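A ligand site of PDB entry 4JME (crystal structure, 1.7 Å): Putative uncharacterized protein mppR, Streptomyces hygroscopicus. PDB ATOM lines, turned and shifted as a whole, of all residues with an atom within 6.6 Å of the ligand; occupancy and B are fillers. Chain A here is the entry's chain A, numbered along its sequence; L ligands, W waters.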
ATOM      1  N   TRP A  56      25.307 -24.485  -3.478  1.00  0.00           N
ATOM      2  CA  TRP A  56      25.352 -25.917  -3.645  1.00  0.00           C
ATOM      3  C   TRP A  56      26.390 -26.213  -4.714  1.00  0.00           C
ATOM      4  O   TRP A  56      26.473 -25.502  -5.725  1.00  0.00           O
ATOM      5  CB  TRP A  56      23.989 -26.499  -4.094  1.00  0.00           C
ATOM      6  CG  TRP A  56      22.818 -26.041  -3.260  1.00  0.00           C
ATOM      7  CD1 TRP A  56      22.603 -26.286  -1.944  1.00  0.00           C
ATOM      8  CD2 TRP A  56      21.702 -25.273  -3.709  1.00  0.00           C
ATOM      9  NE1 TRP A  56      21.418 -25.700  -1.536  1.00  0.00           N
ATOM     10  CE2 TRP A  56      20.852 -25.074  -2.608  1.00  0.00           C
ATOM     11  CE3 TRP A  56      21.342 -24.695  -4.936  1.00  0.00           C
ATOM     12  CZ2 TRP A  56      19.671 -24.339  -2.696  1.00  0.00           C
ATOM     13  CZ3 TRP A  56      20.154 -24.001  -5.037  1.00  0.00           C
ATOM     14  CH2 TRP A  56      19.337 -23.825  -3.908  1.00  0.00           C
ATOM     15  N   PHE A  58      27.965 -28.989  -7.463  1.00  0.00           N
ATOM     16  CA  PHE A  58      27.575 -30.087  -8.344  1.00  0.00           C
ATOM     17  C   PHE A  58      28.791 -30.661  -9.061  1.00  0.00           C
ATOM     18  O   PHE A  58      29.657 -29.908  -9.527  1.00  0.00           O
ATOM     19  CB  PHE A  58      26.590 -29.587  -9.402  1.00  0.00           C
ATOM     20  CG  PHE A  58      25.301 -29.104  -8.841  1.00  0.00           C
ATOM     21  CD1 PHE A  58      25.171 -27.830  -8.349  1.00  0.00           C
ATOM     22  CD2 PHE A  58      24.207 -29.970  -8.782  1.00  0.00           C
ATOM     23  CE1 PHE A  58      23.971 -27.407  -7.811  1.00  0.00           C
ATOM     24  CE2 PHE A  58      23.007 -29.548  -8.244  1.00  0.00           C
ATOM     25  CZ  PHE A  58      22.882 -28.280  -7.772  1.00  0.00           C
ATOM     26  N   ALA A  96      22.367 -36.038 -17.783  1.00  0.00           N
ATOM     27  CA  ALA A  96      23.442 -35.968 -16.813  1.00  0.00           C
ATOM     28  C   ALA A  96      23.141 -36.782 -15.568  1.00  0.00           C
ATOM     29  O   ALA A  96      21.975 -36.949 -15.208  1.00  0.00           O
ATOM     30  CB  ALA A  96      23.704 -34.526 -16.429  1.00  0.00           C
ATOM     31  N   TRP A  98      24.368 -36.570 -11.538  1.00  0.00           N
ATOM     32  CA  TRP A  98      24.975 -35.618 -10.628  1.00  0.00           C
ATOM     33  C   TRP A  98      25.194 -36.165  -9.251  1.00  0.00           C
ATOM     34  O   TRP A  98      24.410 -37.003  -8.781  1.00  0.00           O
ATOM     35  CB  TRP A  98      24.077 -34.386 -10.456  1.00  0.00           C
ATOM     36  CG  TRP A  98      23.792 -33.639 -11.716  1.00  0.00           C
ATOM     37  CD1 TRP A  98      22.626 -33.660 -12.429  1.00  0.00           C
ATOM     38  CD2 TRP A  98      24.669 -32.741 -12.405  1.00  0.00           C
ATOM     39  NE1 TRP A  98      22.736 -32.831 -13.527  1.00  0.00           N
ATOM     40  CE2 TRP A  98      23.976 -32.257 -13.528  1.00  0.00           C
ATOM     41  CE3 TRP A  98      25.963 -32.297 -12.169  1.00  0.00           C
ATOM     42  CZ2 TRP A  98      24.544 -31.360 -14.437  1.00  0.00           C
ATOM     43  CZ3 TRP A  98      26.530 -31.400 -13.078  1.00  0.00           C
ATOM     44  CH2 TRP A  98      25.812 -30.943 -14.193  1.00  0.00           C
ATOM     45  N   TRP A 100      25.605 -33.816  -5.667  1.00  0.00           N
ATOM     46  CA  TRP A 100      25.568 -32.451  -5.194  1.00  0.00           C
ATOM     47  C   TRP A 100      25.754 -32.442  -3.690  1.00  0.00           C
ATOM     48  O   TRP A 100      25.569 -33.458  -2.994  1.00  0.00           O
ATOM     49  CB  TRP A 100      24.215 -31.783  -5.543  1.00  0.00           C
ATOM     50  CG  TRP A 100      23.061 -32.430  -4.807  1.00  0.00           C
ATOM     51  CD1 TRP A 100      22.311 -33.500  -5.207  1.00  0.00           C
ATOM     52  CD2 TRP A 100      22.542 -32.029  -3.535  1.00  0.00           C
ATOM     53  NE1 TRP A 100      21.378 -33.817  -4.239  1.00  0.00           N
ATOM     54  CE2 TRP A 100      21.500 -32.922  -3.212  1.00  0.00           C
ATOM     55  CE3 TRP A 100      22.883 -31.027  -2.629  1.00  0.00           C
ATOM     56  CZ2 TRP A 100      20.780 -32.811  -2.014  1.00  0.00           C
ATOM     57  CZ3 TRP A 100      22.167 -30.937  -1.433  1.00  0.00           C
ATOM     58  CH2 TRP A 100      21.142 -31.821  -1.152  1.00  0.00           C
ATOM     59  N   PHE A 116      21.419 -37.685  -8.249  1.00  0.00           N
ATOM     60  CA  PHE A 116      20.217 -37.746  -9.106  1.00  0.00           C
ATOM     61  C   PHE A 116      20.583 -37.759 -10.575  1.00  0.00           C
ATOM     62  O   PHE A 116      21.672 -37.344 -10.964  1.00  0.00           O
ATOM     63  CB  PHE A 116      19.254 -36.594  -8.811  1.00  0.00           C
ATOM     64  CG  PHE A 116      19.760 -35.220  -9.207  1.00  0.00           C
ATOM     65  CD1 PHE A 116      20.651 -34.542  -8.401  1.00  0.00           C
ATOM     66  CD2 PHE A 116      19.300 -34.591 -10.348  1.00  0.00           C
ATOM     67  CE1 PHE A 116      21.107 -33.262  -8.740  1.00  0.00           C
ATOM     68  CE2 PHE A 116      19.733 -33.323 -10.699  1.00  0.00           C
ATOM     69  CZ  PHE A 116      20.623 -32.631  -9.888  1.00  0.00           C
ATOM     70  N   GLU A 118      19.167 -36.596 -14.595  1.00  0.00           N
ATOM     71  CA  GLU A 118      18.505 -35.408 -15.144  1.00  0.00           C
ATOM     72  C   GLU A 118      18.514 -35.466 -16.664  1.00  0.00           C
ATOM     73  O   GLU A 118      19.475 -35.971 -17.271  1.00  0.00           O
ATOM     74  CB  GLU A 118      19.258 -34.154 -14.689  1.00  0.00           C
ATOM     75  CG  GLU A 118      18.694 -32.828 -15.145  1.00  0.00           C
ATOM     76  CD  GLU A 118      19.603 -31.709 -14.644  1.00  0.00           C
ATOM     77  OE1 GLU A 118      19.225 -31.033 -13.652  1.00  0.00           O
ATOM     78  OE2 GLU A 118      20.715 -31.577 -15.203  1.00  0.00           O
ATOM     79  N   LEU A 120      17.533 -32.557 -19.784  1.00  0.00           N
ATOM     80  CA  LEU A 120      17.132 -31.194 -20.065  1.00  0.00           C
ATOM     81  C   LEU A 120      17.112 -30.944 -21.563  1.00  0.00           C
ATOM     82  O   LEU A 120      17.880 -31.530 -22.294  1.00  0.00           O
ATOM     83  CB  LEU A 120      18.161 -30.184 -19.511  1.00  0.00           C
ATOM     84  CG  LEU A 120      18.680 -30.164 -18.093  1.00  0.00           C
ATOM     85  CD1 LEU A 120      19.689 -29.077 -17.949  1.00  0.00           C
ATOM     86  CD2 LEU A 120      17.540 -29.948 -17.134  1.00  0.00           C
ATOM     87  N   VAL A 140      13.940 -34.844 -13.577  1.00  0.00           N
ATOM     88  CA  VAL A 140      14.855 -35.466 -12.648  1.00  0.00           C
ATOM     89  C   VAL A 140      14.181 -36.655 -11.991  1.00  0.00           C
ATOM     90  O   VAL A 140      12.971 -36.844 -12.145  1.00  0.00           O
ATOM     91  CB  VAL A 140      15.360 -34.523 -11.553  1.00  0.00           C
ATOM     92  CG1 VAL A 140      16.236 -33.417 -12.153  1.00  0.00           C
ATOM     93  CG2 VAL A 140      14.197 -33.931 -10.754  1.00  0.00           C
ATOM     94  N   VAL A 144      14.191 -33.864  -3.971  1.00  0.00           N
ATOM     95  CA  VAL A 144      14.888 -32.641  -3.546  1.00  0.00           C
ATOM     96  C   VAL A 144      15.351 -31.838  -4.751  1.00  0.00           C
ATOM     97  O   VAL A 144      15.094 -30.637  -4.832  1.00  0.00           O
ATOM     98  CB  VAL A 144      16.021 -32.931  -2.533  1.00  0.00           C
ATOM     99  CG1 VAL A 144      17.046 -31.781  -2.436  1.00  0.00           C
ATOM    100  CG2 VAL A 144      15.407 -33.230  -1.129  1.00  0.00           C
ATOM    101  N   PRO A 145      16.040 -32.467  -5.705  1.00  0.00           N
ATOM    102  CA  PRO A 145      16.442 -31.680  -6.878  1.00  0.00           C
ATOM    103  C   PRO A 145      15.267 -31.131  -7.659  1.00  0.00           C
ATOM    104  O   PRO A 145      15.373 -30.036  -8.219  1.00  0.00           O
ATOM    105  CB  PRO A 145      17.242 -32.668  -7.721  1.00  0.00           C
ATOM    106  CG  PRO A 145      17.761 -33.673  -6.756  1.00  0.00           C
ATOM    107  CD  PRO A 145      16.774 -33.732  -5.599  1.00  0.00           C
ATOM    108  N   MET A 146      14.158 -31.854  -7.703  1.00  0.00           N
ATOM    109  CA  MET A 146      12.974 -31.334  -8.388  1.00  0.00           C
ATOM    110  C   MET A 146      12.479 -30.034  -7.753  1.00  0.00           C
ATOM    111  O   MET A 146      12.296 -29.031  -8.446  1.00  0.00           O
ATOM    112  CB  MET A 146      11.835 -32.348  -8.428  1.00  0.00           C
ATOM    113  CG  MET A 146      10.673 -31.858  -9.273  1.00  0.00           C
ATOM    114  SD  MET A 146       9.312 -33.053  -9.279  1.00  0.00           S
ATOM    115  CE  MET A 146       8.611 -32.681  -7.681  1.00  0.00           C
ATOM    116  N   ARG A 148      14.077 -28.054  -5.699  1.00  0.00           N
ATOM    117  CA  ARG A 148      15.124 -27.060  -5.767  1.00  0.00           C
ATOM    118  C   ARG A 148      15.127 -26.398  -7.146  1.00  0.00           C
ATOM    119  O   ARG A 148      15.407 -25.208  -7.278  1.00  0.00           O
ATOM    120  CB  ARG A 148      16.486 -27.692  -5.472  1.00  0.00           C
ATOM    121  CG  ARG A 148      17.558 -26.682  -5.132  1.00  0.00           C
ATOM    122  CD  ARG A 148      18.766 -27.339  -4.519  1.00  0.00           C
ATOM    123  NE  ARG A 148      19.270 -28.424  -5.344  1.00  0.00           N
ATOM    124  CZ  ARG A 148      19.812 -29.546  -4.871  1.00  0.00           C
ATOM    125  NH1 ARG A 148      19.954 -29.725  -3.559  1.00  0.00           N
ATOM    126  NH2 ARG A 148      20.204 -30.476  -5.727  1.00  0.00           N
ATOM    127  N   GLY A 149      14.820 -27.174  -8.184  1.00  0.00           N
ATOM    128  CA  GLY A 149      14.688 -26.612  -9.508  1.00  0.00           C
ATOM    129  C   GLY A 149      13.640 -25.515  -9.566  1.00  0.00           C
ATOM    130  O   GLY A 149      13.907 -24.406 -10.109  1.00  0.00           O
ATOM    131  N   GLN A 152      14.672 -22.140  -8.356  1.00  0.00           N
ATOM    132  CA  GLN A 152      15.523 -21.411  -9.308  1.00  0.00           C
ATOM    133  C   GLN A 152      14.782 -21.000 -10.565  1.00  0.00           C
ATOM    134  O   GLN A 152      15.333 -20.305 -11.404  1.00  0.00           O
ATOM    135  CB  GLN A 152      16.686 -22.270  -9.779  1.00  0.00           C
ATOM    136  CG  GLN A 152      17.612 -22.835  -8.778  1.00  0.00           C
ATOM    137  CD  GLN A 152      18.191 -24.194  -9.242  1.00  0.00           C
ATOM    138  OE1 GLN A 152      18.136 -25.149  -8.501  1.00  0.00           O
ATOM    139  NE2 GLN A 152      18.730 -24.267 -10.455  1.00  0.00           N
ATOM    140  N   MET A 154      13.825 -23.446 -12.747  1.00  0.00           N
ATOM    141  CA  MET A 154      14.083 -24.524 -13.717  1.00  0.00           C
ATOM    142  C   MET A 154      12.902 -25.483 -13.650  1.00  0.00           C
ATOM    143  O   MET A 154      12.600 -26.011 -12.583  1.00  0.00           O
ATOM    144  CB  MET A 154      15.418 -25.285 -13.488  1.00  0.00           C
ATOM    145  CG  MET A 154      15.734 -26.321 -14.662  1.00  0.00           C
ATOM    146  SD  MET A 154      17.273 -27.344 -14.583  1.00  0.00           S
ATOM    147  CE  MET A 154      18.406 -26.236 -15.420  1.00  0.00           C
ATOM    148  N   LYS A 156      11.606 -28.392 -13.652  1.00  0.00           N
ATOM    149  CA  LYS A 156      11.765 -29.833 -13.451  1.00  0.00           C
ATOM    150  C   LYS A 156      10.480 -30.592 -13.111  1.00  0.00           C
ATOM    151  O   LYS A 156       9.702 -30.187 -12.241  1.00  0.00           O
ATOM    152  CB  LYS A 156      12.799 -30.055 -12.338  1.00  0.00           C
ATOM    153  CG  LYS A 156      14.214 -29.603 -12.643  1.00  0.00           C
ATOM    154  CD  LYS A 156      15.177 -29.915 -11.504  1.00  0.00           C
ATOM    155  CE  LYS A 156      16.578 -29.297 -11.650  1.00  0.00           C
ATOM    156  NZ  LYS A 156      17.416 -29.543 -10.427  1.00  0.00           N
ATOM    157  N   HIS A 211      26.223 -25.429 -23.062  1.00  0.00           N
ATOM    158  CA  HIS A 211      26.526 -25.832 -21.705  1.00  0.00           C
ATOM    159  C   HIS A 211      27.545 -24.873 -21.078  1.00  0.00           C
ATOM    160  O   HIS A 211      28.025 -25.148 -19.971  1.00  0.00           O
ATOM    161  CB  HIS A 211      27.080 -27.262 -21.661  1.00  0.00           C
ATOM    162  CG  HIS A 211      26.699 -28.003 -20.425  1.00  0.00           C
ATOM    163  ND1 HIS A 211      27.150 -27.654 -19.169  1.00  0.00           N
ATOM    164  CD2 HIS A 211      25.895 -29.085 -20.239  1.00  0.00           C
ATOM    165  CE1 HIS A 211      26.621 -28.472 -18.262  1.00  0.00           C
ATOM    166  NE2 HIS A 211      25.874 -29.357 -18.892  1.00  0.00           N
ATOM    167  N   LEU A 215      22.008 -19.752 -17.782  1.00  0.00           N
ATOM    168  CA  LEU A 215      20.631 -20.177 -17.965  1.00  0.00           C
ATOM    169  C   LEU A 215      19.670 -19.090 -17.456  1.00  0.00           C
ATOM    170  O   LEU A 215      19.827 -18.575 -16.336  1.00  0.00           O
ATOM    171  CB  LEU A 215      20.383 -21.445 -17.175  1.00  0.00           C
ATOM    172  CG  LEU A 215      21.296 -22.628 -17.478  1.00  0.00           C
ATOM    173  CD1 LEU A 215      20.916 -23.828 -16.592  1.00  0.00           C
ATOM    174  CD2 LEU A 215      21.214 -22.962 -18.943  1.00  0.00           C
ATOM    175  N   TYR A 281      31.505 -32.396 -15.594  1.00  0.00           N
ATOM    176  CA  TYR A 281      31.209 -30.970 -15.417  1.00  0.00           C
ATOM    177  C   TYR A 281      31.036 -30.679 -13.945  1.00  0.00           C
ATOM    178  O   TYR A 281      30.437 -31.472 -13.218  1.00  0.00           O
ATOM    179  CB  TYR A 281      29.904 -30.620 -16.117  1.00  0.00           C
ATOM    180  CG  TYR A 281      29.477 -29.180 -15.942  1.00  0.00           C
ATOM    181  CD1 TYR A 281      29.995 -28.184 -16.743  1.00  0.00           C
ATOM    182  CD2 TYR A 281      28.597 -28.805 -14.934  1.00  0.00           C
ATOM    183  CE1 TYR A 281      29.591 -26.865 -16.603  1.00  0.00           C
ATOM    184  CE2 TYR A 281      28.201 -27.499 -14.778  1.00  0.00           C
ATOM    185  CZ  TYR A 281      28.716 -26.525 -15.601  1.00  0.00           C
ATOM    186  OH  TYR A 281      28.312 -25.206 -15.461  1.00  0.00           O
ATOM    187  N   GLU A 283      30.201 -27.202 -11.088  1.00  0.00           N
ATOM    188  CA  GLU A 283      29.898 -25.797 -10.876  1.00  0.00           C
ATOM    189  C   GLU A 283      29.423 -25.638  -9.434  1.00  0.00           C
ATOM    190  O   GLU A 283      29.032 -26.615  -8.761  1.00  0.00           O
ATOM    191  CB  GLU A 283      28.806 -25.285 -11.827  1.00  0.00           C
ATOM    192  CG  GLU A 283      27.437 -25.828 -11.531  1.00  0.00           C
ATOM    193  CD  GLU A 283      26.296 -25.260 -12.397  1.00  0.00           C
ATOM    194  OE1 GLU A 283      25.152 -25.289 -11.917  1.00  0.00           O
ATOM    195  OE2 GLU A 283      26.533 -24.798 -13.543  1.00  0.00           O
ATOM    196  N   LEU A 285      26.584 -23.291  -7.482  1.00  0.00           N
ATOM    197  CA  LEU A 285      25.382 -22.508  -7.784  1.00  0.00           C
ATOM    198  C   LEU A 285      25.028 -21.686  -6.552  1.00  0.00           C
ATOM    199  O   LEU A 285      24.850 -22.239  -5.475  1.00  0.00           O
ATOM    200  CB  LEU A 285      24.255 -23.466  -8.173  1.00  0.00           C
ATOM    201  CG  LEU A 285      22.870 -22.887  -8.470  1.00  0.00           C
ATOM    202  CD1 LEU A 285      22.936 -21.913  -9.621  1.00  0.00           C
ATOM    203  CD2 LEU A 285      21.868 -24.011  -8.757  1.00  0.00           C
HETATM  204  O1  LIG L   1      19.282 -27.814  -8.098  1.00  0.00           O
HETATM  205  C1  LIG L   1      18.994 -28.825  -8.726  1.00  0.00           C
HETATM  206  O2  LIG L   1      19.201 -29.952  -8.204  1.00  0.00           O
HETATM  207  C2  LIG L   1      18.392 -28.700 -10.086  1.00  0.00           C
HETATM  208  C3  LIG L   1      19.158 -28.006 -11.162  1.00  0.00           C
HETATM  209  C4  LIG L   1      20.581 -28.448 -11.362  1.00  0.00           C
HETATM  210  C5  LIG L   1      21.503 -27.184 -11.607  1.00  0.00           C
HETATM  211  N1  LIG L   1      21.967 -27.353 -12.985  1.00  0.00           N
HETATM  212  C6  LIG L   1      21.481 -28.525 -13.524  1.00  0.00           C
HETATM  213  N2  LIG L   1      21.723 -28.986 -14.732  1.00  0.00           N
HETATM  214  N3  LIG L   1      20.695 -29.164 -12.620  1.00  0.00           N
HETATM  215  O   HOH W   1      23.270 -29.836 -17.655  1.00  0.00           O
HETATM  216  O   HOH W   2      22.838 -27.168 -17.446  1.00  0.00           O
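C2 of the ligand is covalently linked to NZ of Lys 156, 1.3 Å away. The side-chain carboxylate (OE2) of Glu 118 lies within salt-bridge range of a nitrogen (N2) of the ligand, 2.8 Å away. The guanidinium group (NH2) of Arg 148 is in salt-bridge range of an oxygen (O2) of the ligand. An oxygen (O1) of the ligand sits close to the side-chain amide oxygen (OE1) of Gln 152.
OE1 of Glu 118 is in salt-bridge range of NZ of Lys 156, at 3.99 Å. O of Pro 145 sits at hydrogen-bond distance from NZ of Lys 156 (3.0 Å). The indole nitrogen (NE1) of Trp 98 lies within hydrogen-bond range of the side-chain carboxylate (OE2) of Glu 118 (2.9 Å). O of Ala 96 is in hydrogen-bond range of N of Glu 118 (2.9 Å). The backbone carbonyl oxygen of Phe 116 sits at hydrogen-bond distance from the backbone NH of Trp 98, 2.9 Å away. N of Phe 58 is in hydrogen-bond range of O of Glu 283, 2.9 Å away. OE2 of Glu 283 lies within hydrogen-bond range of OH of Tyr 281, at 2.6 Å. The backbone carbonyl oxygen (O) of Gly 149 is in hydrogen-bond range of the backbone NH (N) of Met 154 (2.8 Å).
Merely in contact with the ligand: Phe 58 (3.6 Å), Trp 98 (3.7 Å), Phe 116 (3.5 Å), Leu 120 (3.8 Å), Pro 145 (3.4 Å), Met 154 (3.96 Å) and Glu 283 (3.9 Å). Hydrophobic or aromatic side chains that line the ligand: Phe 58, Trp 98, Phe 116, Leu 120, Pro 145 and Met 154.
Water W1 lies within hydrogen-bond range of NE2 of His 211 (2.9 Å) and N2 of the ligand (3.4 Å).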
